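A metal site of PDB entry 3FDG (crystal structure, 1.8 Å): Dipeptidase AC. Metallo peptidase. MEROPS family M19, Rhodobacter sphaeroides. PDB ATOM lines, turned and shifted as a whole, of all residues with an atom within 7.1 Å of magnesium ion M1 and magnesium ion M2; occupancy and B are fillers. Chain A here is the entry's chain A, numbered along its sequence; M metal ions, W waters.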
ATOM      1  N   HIS A  11      21.511 -22.363  12.947  1.00  0.00           N
ATOM      2  CA  HIS A  11      21.256 -22.608  14.395  1.00  0.00           C
ATOM      3  C   HIS A  11      20.170 -23.640  14.624  1.00  0.00           C
ATOM      4  O   HIS A  11      19.038 -23.458  14.189  1.00  0.00           O
ATOM      5  CB  HIS A  11      20.767 -21.314  15.108  1.00  0.00           C
ATOM      6  CG  HIS A  11      20.666 -21.441  16.615  1.00  0.00           C
ATOM      7  ND1 HIS A  11      21.707 -21.120  17.441  1.00  0.00           N
ATOM      8  CD2 HIS A  11      19.620 -21.786  17.416  1.00  0.00           C
ATOM      9  CE1 HIS A  11      21.332 -21.280  18.710  1.00  0.00           C
ATOM     10  NE2 HIS A  11      20.074 -21.685  18.723  1.00  0.00           N
ATOM     11  N   ASN A  12      20.490 -24.689  15.385  1.00  0.00           N
ATOM     12  CA  ASN A  12      19.428 -25.545  15.905  1.00  0.00           C
ATOM     13  C   ASN A  12      19.735 -25.965  17.319  1.00  0.00           C
ATOM     14  O   ASN A  12      20.908 -25.957  17.751  1.00  0.00           O
ATOM     15  CB  ASN A  12      19.240 -26.784  14.997  1.00  0.00           C
ATOM     16  CG  ASN A  12      20.465 -27.692  14.968  1.00  0.00           C
ATOM     17  OD1 ASN A  12      21.197 -27.842  15.991  1.00  0.00           O
ATOM     18  ND2 ASN A  12      20.724 -28.282  13.817  1.00  0.00           N
ATOM     19  N   ASP A  13      18.686 -26.407  18.025  1.00  0.00           N
ATOM     20  CA  ASP A  13      18.797 -26.807  19.439  1.00  0.00           C
ATOM     21  C   ASP A  13      18.446 -28.270  19.611  1.00  0.00           C
ATOM     22  O   ASP A  13      17.897 -28.710  20.650  1.00  0.00           O
ATOM     23  CB  ASP A  13      17.852 -25.897  20.285  1.00  0.00           C
ATOM     24  CG  ASP A  13      18.383 -24.428  20.379  1.00  0.00           C
ATOM     25  OD1 ASP A  13      19.489 -24.178  20.944  1.00  0.00           O
ATOM     26  OD2 ASP A  13      17.723 -23.524  19.840  1.00  0.00           O
ATOM     27  N   LEU A  16      19.383 -30.046  22.832  1.00  0.00           N
ATOM     28  CA  LEU A  16      18.626 -29.839  24.040  1.00  0.00           C
ATOM     29  C   LEU A  16      17.695 -31.038  24.206  1.00  0.00           C
ATOM     30  O   LEU A  16      17.398 -31.475  25.341  1.00  0.00           O
ATOM     31  CB  LEU A  16      17.907 -28.480  23.934  1.00  0.00           C
ATOM     32  CG  LEU A  16      17.242 -27.944  25.199  1.00  0.00           C
ATOM     33  CD1 LEU A  16      18.246 -27.774  26.353  1.00  0.00           C
ATOM     34  CD2 LEU A  16      16.539 -26.605  24.815  1.00  0.00           C
ATOM     35  N   ALA A  54      23.809 -25.864  18.535  1.00  0.00           N
ATOM     36  CA  ALA A  54      24.019 -25.023  19.766  1.00  0.00           C
ATOM     37  C   ALA A  54      24.086 -25.861  21.015  1.00  0.00           C
ATOM     38  O   ALA A  54      23.194 -26.687  21.280  1.00  0.00           O
ATOM     39  CB  ALA A  54      22.833 -24.095  19.927  1.00  0.00           C
ATOM     40  N   ILE A  55      25.102 -25.564  21.816  1.00  0.00           N
ATOM     41  CA  ILE A  55      25.161 -25.870  23.216  1.00  0.00           C
ATOM     42  C   ILE A  55      24.538 -24.657  23.902  1.00  0.00           C
ATOM     43  O   ILE A  55      25.079 -23.538  23.876  1.00  0.00           O
ATOM     44  CB  ILE A  55      26.593 -26.086  23.699  1.00  0.00           C
ATOM     45  CG1 ILE A  55      27.197 -27.315  22.991  1.00  0.00           C
ATOM     46  CG2 ILE A  55      26.637 -26.236  25.258  1.00  0.00           C
ATOM     47  CD1 ILE A  55      28.726 -27.426  23.097  1.00  0.00           C
ATOM     48  N   TYR A  56      23.390 -24.903  24.521  1.00  0.00           N
ATOM     49  CA  TYR A  56      22.629 -23.855  25.190  1.00  0.00           C
ATOM     50  C   TYR A  56      22.181 -24.375  26.565  1.00  0.00           C
ATOM     51  O   TYR A  56      21.480 -25.406  26.651  1.00  0.00           O
ATOM     52  CB  TYR A  56      21.444 -23.437  24.317  1.00  0.00           C
ATOM     53  CG  TYR A  56      20.319 -22.845  25.096  1.00  0.00           C
ATOM     54  CD1 TYR A  56      20.466 -21.599  25.684  1.00  0.00           C
ATOM     55  CD2 TYR A  56      19.137 -23.574  25.309  1.00  0.00           C
ATOM     56  CE1 TYR A  56      19.449 -21.043  26.456  1.00  0.00           C
ATOM     57  CE2 TYR A  56      18.103 -23.017  26.081  1.00  0.00           C
ATOM     58  CZ  TYR A  56      18.278 -21.764  26.626  1.00  0.00           C
ATOM     59  OH  TYR A  56      17.302 -21.197  27.387  1.00  0.00           O
ATOM     60  N   HIS A 135      28.665 -25.046  18.531  1.00  0.00           N
ATOM     61  CA  HIS A 135      28.315 -23.666  18.790  1.00  0.00           C
ATOM     62  C   HIS A 135      27.846 -23.563  20.232  1.00  0.00           C
ATOM     63  O   HIS A 135      27.225 -24.495  20.768  1.00  0.00           O
ATOM     64  CB  HIS A 135      27.177 -23.214  17.870  1.00  0.00           C
ATOM     65  CG  HIS A 135      26.654 -21.839  18.172  1.00  0.00           C
ATOM     66  ND1 HIS A 135      25.465 -21.592  18.842  1.00  0.00           N
ATOM     67  CD2 HIS A 135      27.165 -20.638  17.858  1.00  0.00           C
ATOM     68  CE1 HIS A 135      25.286 -20.289  18.960  1.00  0.00           C
ATOM     69  NE2 HIS A 135      26.306 -19.683  18.355  1.00  0.00           N
ATOM     70  N   GLU A 137      25.598 -21.102  22.736  1.00  0.00           N
ATOM     71  CA  GLU A 137      24.629 -19.975  22.706  1.00  0.00           C
ATOM     72  C   GLU A 137      24.528 -19.442  24.119  1.00  0.00           C
ATOM     73  O   GLU A 137      23.876 -20.077  24.975  1.00  0.00           O
ATOM     74  CB  GLU A 137      23.263 -20.514  22.208  1.00  0.00           C
ATOM     75  CG  GLU A 137      22.080 -19.497  22.284  1.00  0.00           C
ATOM     76  CD  GLU A 137      20.803 -19.944  21.587  1.00  0.00           C
ATOM     77  OE1 GLU A 137      20.520 -21.138  21.482  1.00  0.00           O
ATOM     78  OE2 GLU A 137      20.032 -19.088  21.127  1.00  0.00           O
ATOM     79  N   TRP A 164      22.701 -15.370  25.770  1.00  0.00           N
ATOM     80  CA  TRP A 164      21.376 -15.758  25.359  1.00  0.00           C
ATOM     81  C   TRP A 164      20.514 -14.597  25.906  1.00  0.00           C
ATOM     82  O   TRP A 164      21.045 -13.470  26.175  1.00  0.00           O
ATOM     83  CB  TRP A 164      20.999 -17.149  26.000  1.00  0.00           C
ATOM     84  CG  TRP A 164      19.602 -17.585  25.622  1.00  0.00           C
ATOM     85  CD1 TRP A 164      19.148 -17.882  24.346  1.00  0.00           C
ATOM     86  CD2 TRP A 164      18.473 -17.732  26.492  1.00  0.00           C
ATOM     87  NE1 TRP A 164      17.782 -18.183  24.404  1.00  0.00           N
ATOM     88  CE2 TRP A 164      17.370 -18.123  25.697  1.00  0.00           C
ATOM     89  CE3 TRP A 164      18.288 -17.589  27.875  1.00  0.00           C
ATOM     90  CZ2 TRP A 164      16.087 -18.370  26.238  1.00  0.00           C
ATOM     91  CZ3 TRP A 164      16.999 -17.844  28.414  1.00  0.00           C
ATOM     92  CH2 TRP A 164      15.921 -18.199  27.580  1.00  0.00           C
ATOM     93  N   SER A 165      19.208 -14.805  26.049  1.00  0.00           N
ATOM     94  CA  SER A 165      18.304 -13.732  26.496  1.00  0.00           C
ATOM     95  C   SER A 165      18.281 -13.825  28.026  1.00  0.00           C
ATOM     96  O   SER A 165      17.308 -14.322  28.608  1.00  0.00           O
ATOM     97  CB  SER A 165      16.935 -13.882  25.787  1.00  0.00           C
ATOM     98  OG  SER A 165      16.979 -13.260  24.454  1.00  0.00           O
ATOM     99  N   PHE A 176      12.709 -11.164  25.616  1.00  0.00           N
ATOM    100  CA  PHE A 176      11.758 -11.356  24.537  1.00  0.00           C
ATOM    101  C   PHE A 176      10.593 -10.382  24.741  1.00  0.00           C
ATOM    102  O   PHE A 176       9.944 -10.409  25.780  1.00  0.00           O
ATOM    103  CB  PHE A 176      11.214 -12.777  24.549  1.00  0.00           C
ATOM    104  CG  PHE A 176      12.301 -13.818  24.401  1.00  0.00           C
ATOM    105  CD1 PHE A 176      13.004 -13.959  23.182  1.00  0.00           C
ATOM    106  CD2 PHE A 176      12.655 -14.630  25.485  1.00  0.00           C
ATOM    107  CE1 PHE A 176      14.069 -14.896  23.063  1.00  0.00           C
ATOM    108  CE2 PHE A 176      13.686 -15.556  25.378  1.00  0.00           C
ATOM    109  CZ  PHE A 176      14.383 -15.704  24.157  1.00  0.00           C
ATOM    110  N   ASP A 207      28.675 -14.766  17.625  1.00  0.00           N
ATOM    111  CA  ASP A 207      27.281 -14.763  17.166  1.00  0.00           C
ATOM    112  C   ASP A 207      26.542 -13.674  17.952  1.00  0.00           C
ATOM    113  O   ASP A 207      26.511 -13.707  19.199  1.00  0.00           O
ATOM    114  CB  ASP A 207      26.633 -16.153  17.322  1.00  0.00           C
ATOM    115  CG  ASP A 207      25.148 -16.157  16.936  1.00  0.00           C
ATOM    116  OD1 ASP A 207      24.674 -15.154  16.371  1.00  0.00           O
ATOM    117  OD2 ASP A 207      24.430 -17.157  17.213  1.00  0.00           O
ATOM    118  N   SER A 209      23.258 -12.845  17.746  1.00  0.00           N
ATOM    119  CA  SER A 209      21.839 -13.132  18.008  1.00  0.00           C
ATOM    120  C   SER A 209      21.654 -13.217  19.525  1.00  0.00           C
ATOM    121  O   SER A 209      22.433 -13.859  20.223  1.00  0.00           O
ATOM    122  CB  SER A 209      21.345 -14.439  17.331  1.00  0.00           C
ATOM    123  OG  SER A 209      21.304 -14.288  15.896  1.00  0.00           O
ATOM    124  N   HIS A 210      20.589 -12.581  19.985  1.00  0.00           N
ATOM    125  CA  HIS A 210      20.242 -12.378  21.431  1.00  0.00           C
ATOM    126  C   HIS A 210      20.958 -11.211  22.073  1.00  0.00           C
ATOM    127  O   HIS A 210      20.525 -10.673  23.117  1.00  0.00           O
ATOM    128  CB  HIS A 210      20.477 -13.628  22.313  1.00  0.00           C
ATOM    129  CG  HIS A 210      19.567 -14.769  21.974  1.00  0.00           C
ATOM    130  ND1 HIS A 210      18.294 -14.876  22.499  1.00  0.00           N
ATOM    131  CD2 HIS A 210      19.734 -15.822  21.139  1.00  0.00           C
ATOM    132  CE1 HIS A 210      17.714 -15.963  22.008  1.00  0.00           C
ATOM    133  NE2 HIS A 210      18.582 -16.575  21.219  1.00  0.00           N
ATOM    134  N   THR A 230      23.388 -15.408  13.780  1.00  0.00           N
ATOM    135  CA  THR A 230      23.034 -16.715  13.173  1.00  0.00           C
ATOM    136  C   THR A 230      21.546 -16.963  13.067  1.00  0.00           C
ATOM    137  O   THR A 230      21.125 -17.799  12.253  1.00  0.00           O
ATOM    138  CB  THR A 230      23.631 -17.894  13.993  1.00  0.00           C
ATOM    139  OG1 THR A 230      23.079 -17.870  15.332  1.00  0.00           O
ATOM    140  CG2 THR A 230      25.171 -17.812  14.051  1.00  0.00           C
ATOM    141  N   HIS A 231      20.752 -16.282  13.870  1.00  0.00           N
ATOM    142  CA  HIS A 231      19.316 -16.548  13.827  1.00  0.00           C
ATOM    143  C   HIS A 231      18.472 -15.335  14.219  1.00  0.00           C
ATOM    144  O   HIS A 231      17.868 -15.309  15.304  1.00  0.00           O
ATOM    145  CB  HIS A 231      18.909 -17.894  14.525  1.00  0.00           C
ATOM    146  CG  HIS A 231      19.220 -17.998  16.013  1.00  0.00           C
ATOM    147  ND1 HIS A 231      20.488 -17.900  16.530  1.00  0.00           N
ATOM    148  CD2 HIS A 231      18.416 -18.272  17.061  1.00  0.00           C
ATOM    149  CE1 HIS A 231      20.459 -18.105  17.842  1.00  0.00           C
ATOM    150  NE2 HIS A 231      19.213 -18.356  18.190  1.00  0.00           N
ATOM    151  N   ARG A 242      14.273  -9.150  19.271  1.00  0.00           N
ATOM    152  CA  ARG A 242      15.251 -10.163  18.826  1.00  0.00           C
ATOM    153  C   ARG A 242      15.731  -9.918  17.371  1.00  0.00           C
ATOM    154  O   ARG A 242      16.709 -10.548  16.914  1.00  0.00           O
ATOM    155  CB  ARG A 242      14.624 -11.572  18.950  1.00  0.00           C
ATOM    156  CG  ARG A 242      14.839 -12.221  20.304  1.00  0.00           C
ATOM    157  CD  ARG A 242      16.301 -12.719  20.367  1.00  0.00           C
ATOM    158  NE  ARG A 242      16.532 -13.998  19.697  1.00  0.00           N
ATOM    159  CZ  ARG A 242      17.218 -14.171  18.557  1.00  0.00           C
ATOM    160  NH1 ARG A 242      17.715 -13.119  17.833  1.00  0.00           N
ATOM    161  NH2 ARG A 242      17.399 -15.425  18.129  1.00  0.00           N
ATOM    162  N   ASN A 262      15.653 -16.663  10.922  1.00  0.00           N
ATOM    163  CA  ASN A 262      15.048 -17.451  12.005  1.00  0.00           C
ATOM    164  C   ASN A 262      13.638 -17.814  11.581  1.00  0.00           C
ATOM    165  O   ASN A 262      12.871 -16.951  11.062  1.00  0.00           O
ATOM    166  CB  ASN A 262      15.037 -16.550  13.260  1.00  0.00           C
ATOM    167  CG  ASN A 262      14.780 -17.325  14.573  1.00  0.00           C
ATOM    168  OD1 ASN A 262      13.910 -18.178  14.626  1.00  0.00           O
ATOM    169  ND2 ASN A 262      15.474 -16.923  15.663  1.00  0.00           N
ATOM    170  N   PHE A 267       9.181 -14.117  15.212  1.00  0.00           N
ATOM    171  CA  PHE A 267      10.122 -13.143  14.603  1.00  0.00           C
ATOM    172  C   PHE A 267       9.884 -12.888  13.104  1.00  0.00           C
ATOM    173  O   PHE A 267      10.593 -12.085  12.489  1.00  0.00           O
ATOM    174  CB  PHE A 267      11.582 -13.553  14.857  1.00  0.00           C
ATOM    175  CG  PHE A 267      11.890 -13.876  16.305  1.00  0.00           C
ATOM    176  CD1 PHE A 267      11.265 -13.188  17.366  1.00  0.00           C
ATOM    177  CD2 PHE A 267      12.817 -14.849  16.585  1.00  0.00           C
ATOM    178  CE1 PHE A 267      11.564 -13.510  18.699  1.00  0.00           C
ATOM    179  CE2 PHE A 267      13.150 -15.181  17.906  1.00  0.00           C
ATOM    180  CZ  PHE A 267      12.488 -14.534  18.972  1.00  0.00           C
ATOM    181  N   ASP A 304      16.553 -22.115  13.815  1.00  0.00           N
ATOM    182  CA  ASP A 304      16.114 -22.238  15.229  1.00  0.00           C
ATOM    183  C   ASP A 304      15.268 -23.540  15.298  1.00  0.00           C
ATOM    184  O   ASP A 304      14.397 -23.709  16.176  1.00  0.00           O
ATOM    185  CB  ASP A 304      15.350 -20.986  15.692  1.00  0.00           C
ATOM    186  CG  ASP A 304      15.718 -20.554  17.156  1.00  0.00           C
ATOM    187  OD1 ASP A 304      16.540 -21.224  17.765  1.00  0.00           O
ATOM    188  OD2 ASP A 304      15.173 -19.619  17.707  1.00  0.00           O
ATOM    189  N   PHE A 305      15.551 -24.472  14.400  1.00  0.00           N
ATOM    190  CA  PHE A 305      14.881 -25.831  14.500  1.00  0.00           C
ATOM    191  C   PHE A 305      15.051 -26.390  15.931  1.00  0.00           C
ATOM    192  O   PHE A 305      16.133 -26.249  16.534  1.00  0.00           O
ATOM    193  CB  PHE A 305      15.489 -26.819  13.549  1.00  0.00           C
ATOM    194  CG  PHE A 305      14.909 -26.789  12.137  1.00  0.00           C
ATOM    195  CD1 PHE A 305      13.518 -26.642  11.923  1.00  0.00           C
ATOM    196  CD2 PHE A 305      15.783 -26.913  11.018  1.00  0.00           C
ATOM    197  CE1 PHE A 305      12.998 -26.594  10.572  1.00  0.00           C
ATOM    198  CE2 PHE A 305      15.279 -26.908   9.733  1.00  0.00           C
ATOM    199  CZ  PHE A 305      13.924 -26.753   9.493  1.00  0.00           C
ATOM    200  N   ASP A 306      13.991 -26.956  16.491  1.00  0.00           N
ATOM    201  CA  ASP A 306      13.945 -27.444  17.874  1.00  0.00           C
ATOM    202  C   ASP A 306      14.154 -26.403  18.975  1.00  0.00           C
ATOM    203  O   ASP A 306      14.307 -26.779  20.145  1.00  0.00           O
ATOM    204  CB  ASP A 306      14.866 -28.674  18.082  1.00  0.00           C
ATOM    205  CG  ASP A 306      14.271 -29.930  17.427  1.00  0.00           C
ATOM    206  OD1 ASP A 306      13.042 -30.079  17.503  1.00  0.00           O
ATOM    207  OD2 ASP A 306      14.993 -30.726  16.812  1.00  0.00           O
ATOM    208  N   GLY A 307      14.159 -25.122  18.600  1.00  0.00           N
ATOM    209  CA  GLY A 307      14.258 -24.026  19.570  1.00  0.00           C
ATOM    210  C   GLY A 307      13.118 -23.012  19.468  1.00  0.00           C
ATOM    211  O   GLY A 307      13.162 -22.057  20.193  1.00  0.00           O
HETATM  212 MG    MG M   1      18.288 -18.545  20.297  1.00  0.00          MG
HETATM  213 MG    MG M   2      19.081 -22.122  20.569  1.00  0.00          MG
HETATM  214  O   HOH W   1      17.670 -20.645  19.957  1.00  0.00           O
HETATM  215  O   HOH W   2      16.944 -19.013  22.290  1.00  0.00           O
HETATM  216  O   HOH W   3      16.248 -18.057  19.558  1.00  0.00           O
HETATM  217  O   HOH W   4      18.138 -21.970  22.415  1.00  0.00           O
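N of Glu 137 lies within hydrogen-bond range of O of Ile 55, at 2.7 Å. The backbone NH (N) of Asp 13 is in hydrogen-bond range of the backbone carbonyl oxygen (O) of Phe 305 (3.0 Å). NE of Arg 242 lies close to ND1 of His 210 (3.4 Å). O of His 231 sits at hydrogen-bond distance from ND2 of Asn 262, at 2.9 Å. N of His 231 sits at hydrogen-bond distance from OG of Ser 209, 2.9 Å away. The side-chain hydroxyl (OG1) of Thr 230 is in hydrogen-bond range of a ring nitrogen (ND1) of His 231. OD2 of Asp 304 sits at hydrogen-bond distance from ND2 of Asn 262 (3.4 Å). The side-chain amide nitrogen (ND2) of Asn 262 lies close to the guanidinium group (NH2) of Arg 242, 3.5 Å away.
Merely in contact with magnesium ion M1: Arg 242 (3.9 Å). Of the 24 residues printed, 5 come within 4 Å of magnesium ion M1.
Residues that only touch magnesium ion M2: Asp 304 (3.9 Å). Four residues have an atom within 4 Å of magnesium ion M2: His 11, Asp 13, Glu 137 and Asp 304.
OE2 of Glu 137 is bound to magnesium ion M1 (2.0 Å). A ring nitrogen (NE2) of His 210 is bound to magnesium ion M1 (2.2 Å). Water W1 is bound to magnesium ion M1, 2.2 Å away. Water W3 is bound to magnesium ion M1. Magnesium ion M1 is bound by NE2 of His 231 (2.3 Å). Water W2 binds magnesium ion M1 (2.4 Å).
OE1 of Glu 137 is bound to magnesium ion M2 (2.0 Å). Water W4 binds magnesium ion M2 (2.1 Å). OD2 of Asp 13 binds magnesium ion M2. Magnesium ion M2 is bound by OD1 of Asp 13, at 2.1 Å. Magnesium ion M2 is bound by water W1, at 2.1 Å. A ring nitrogen (NE2) of His 11 binds magnesium ion M2 (2.1 Å). Magnesium ion M2 has six donor atoms within binding distance.
Water W3 lies within hydrogen-bond range of the side-chain carboxylate (OD2) of Asp 304 and the guanidinium group (NH2) of Arg 242.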
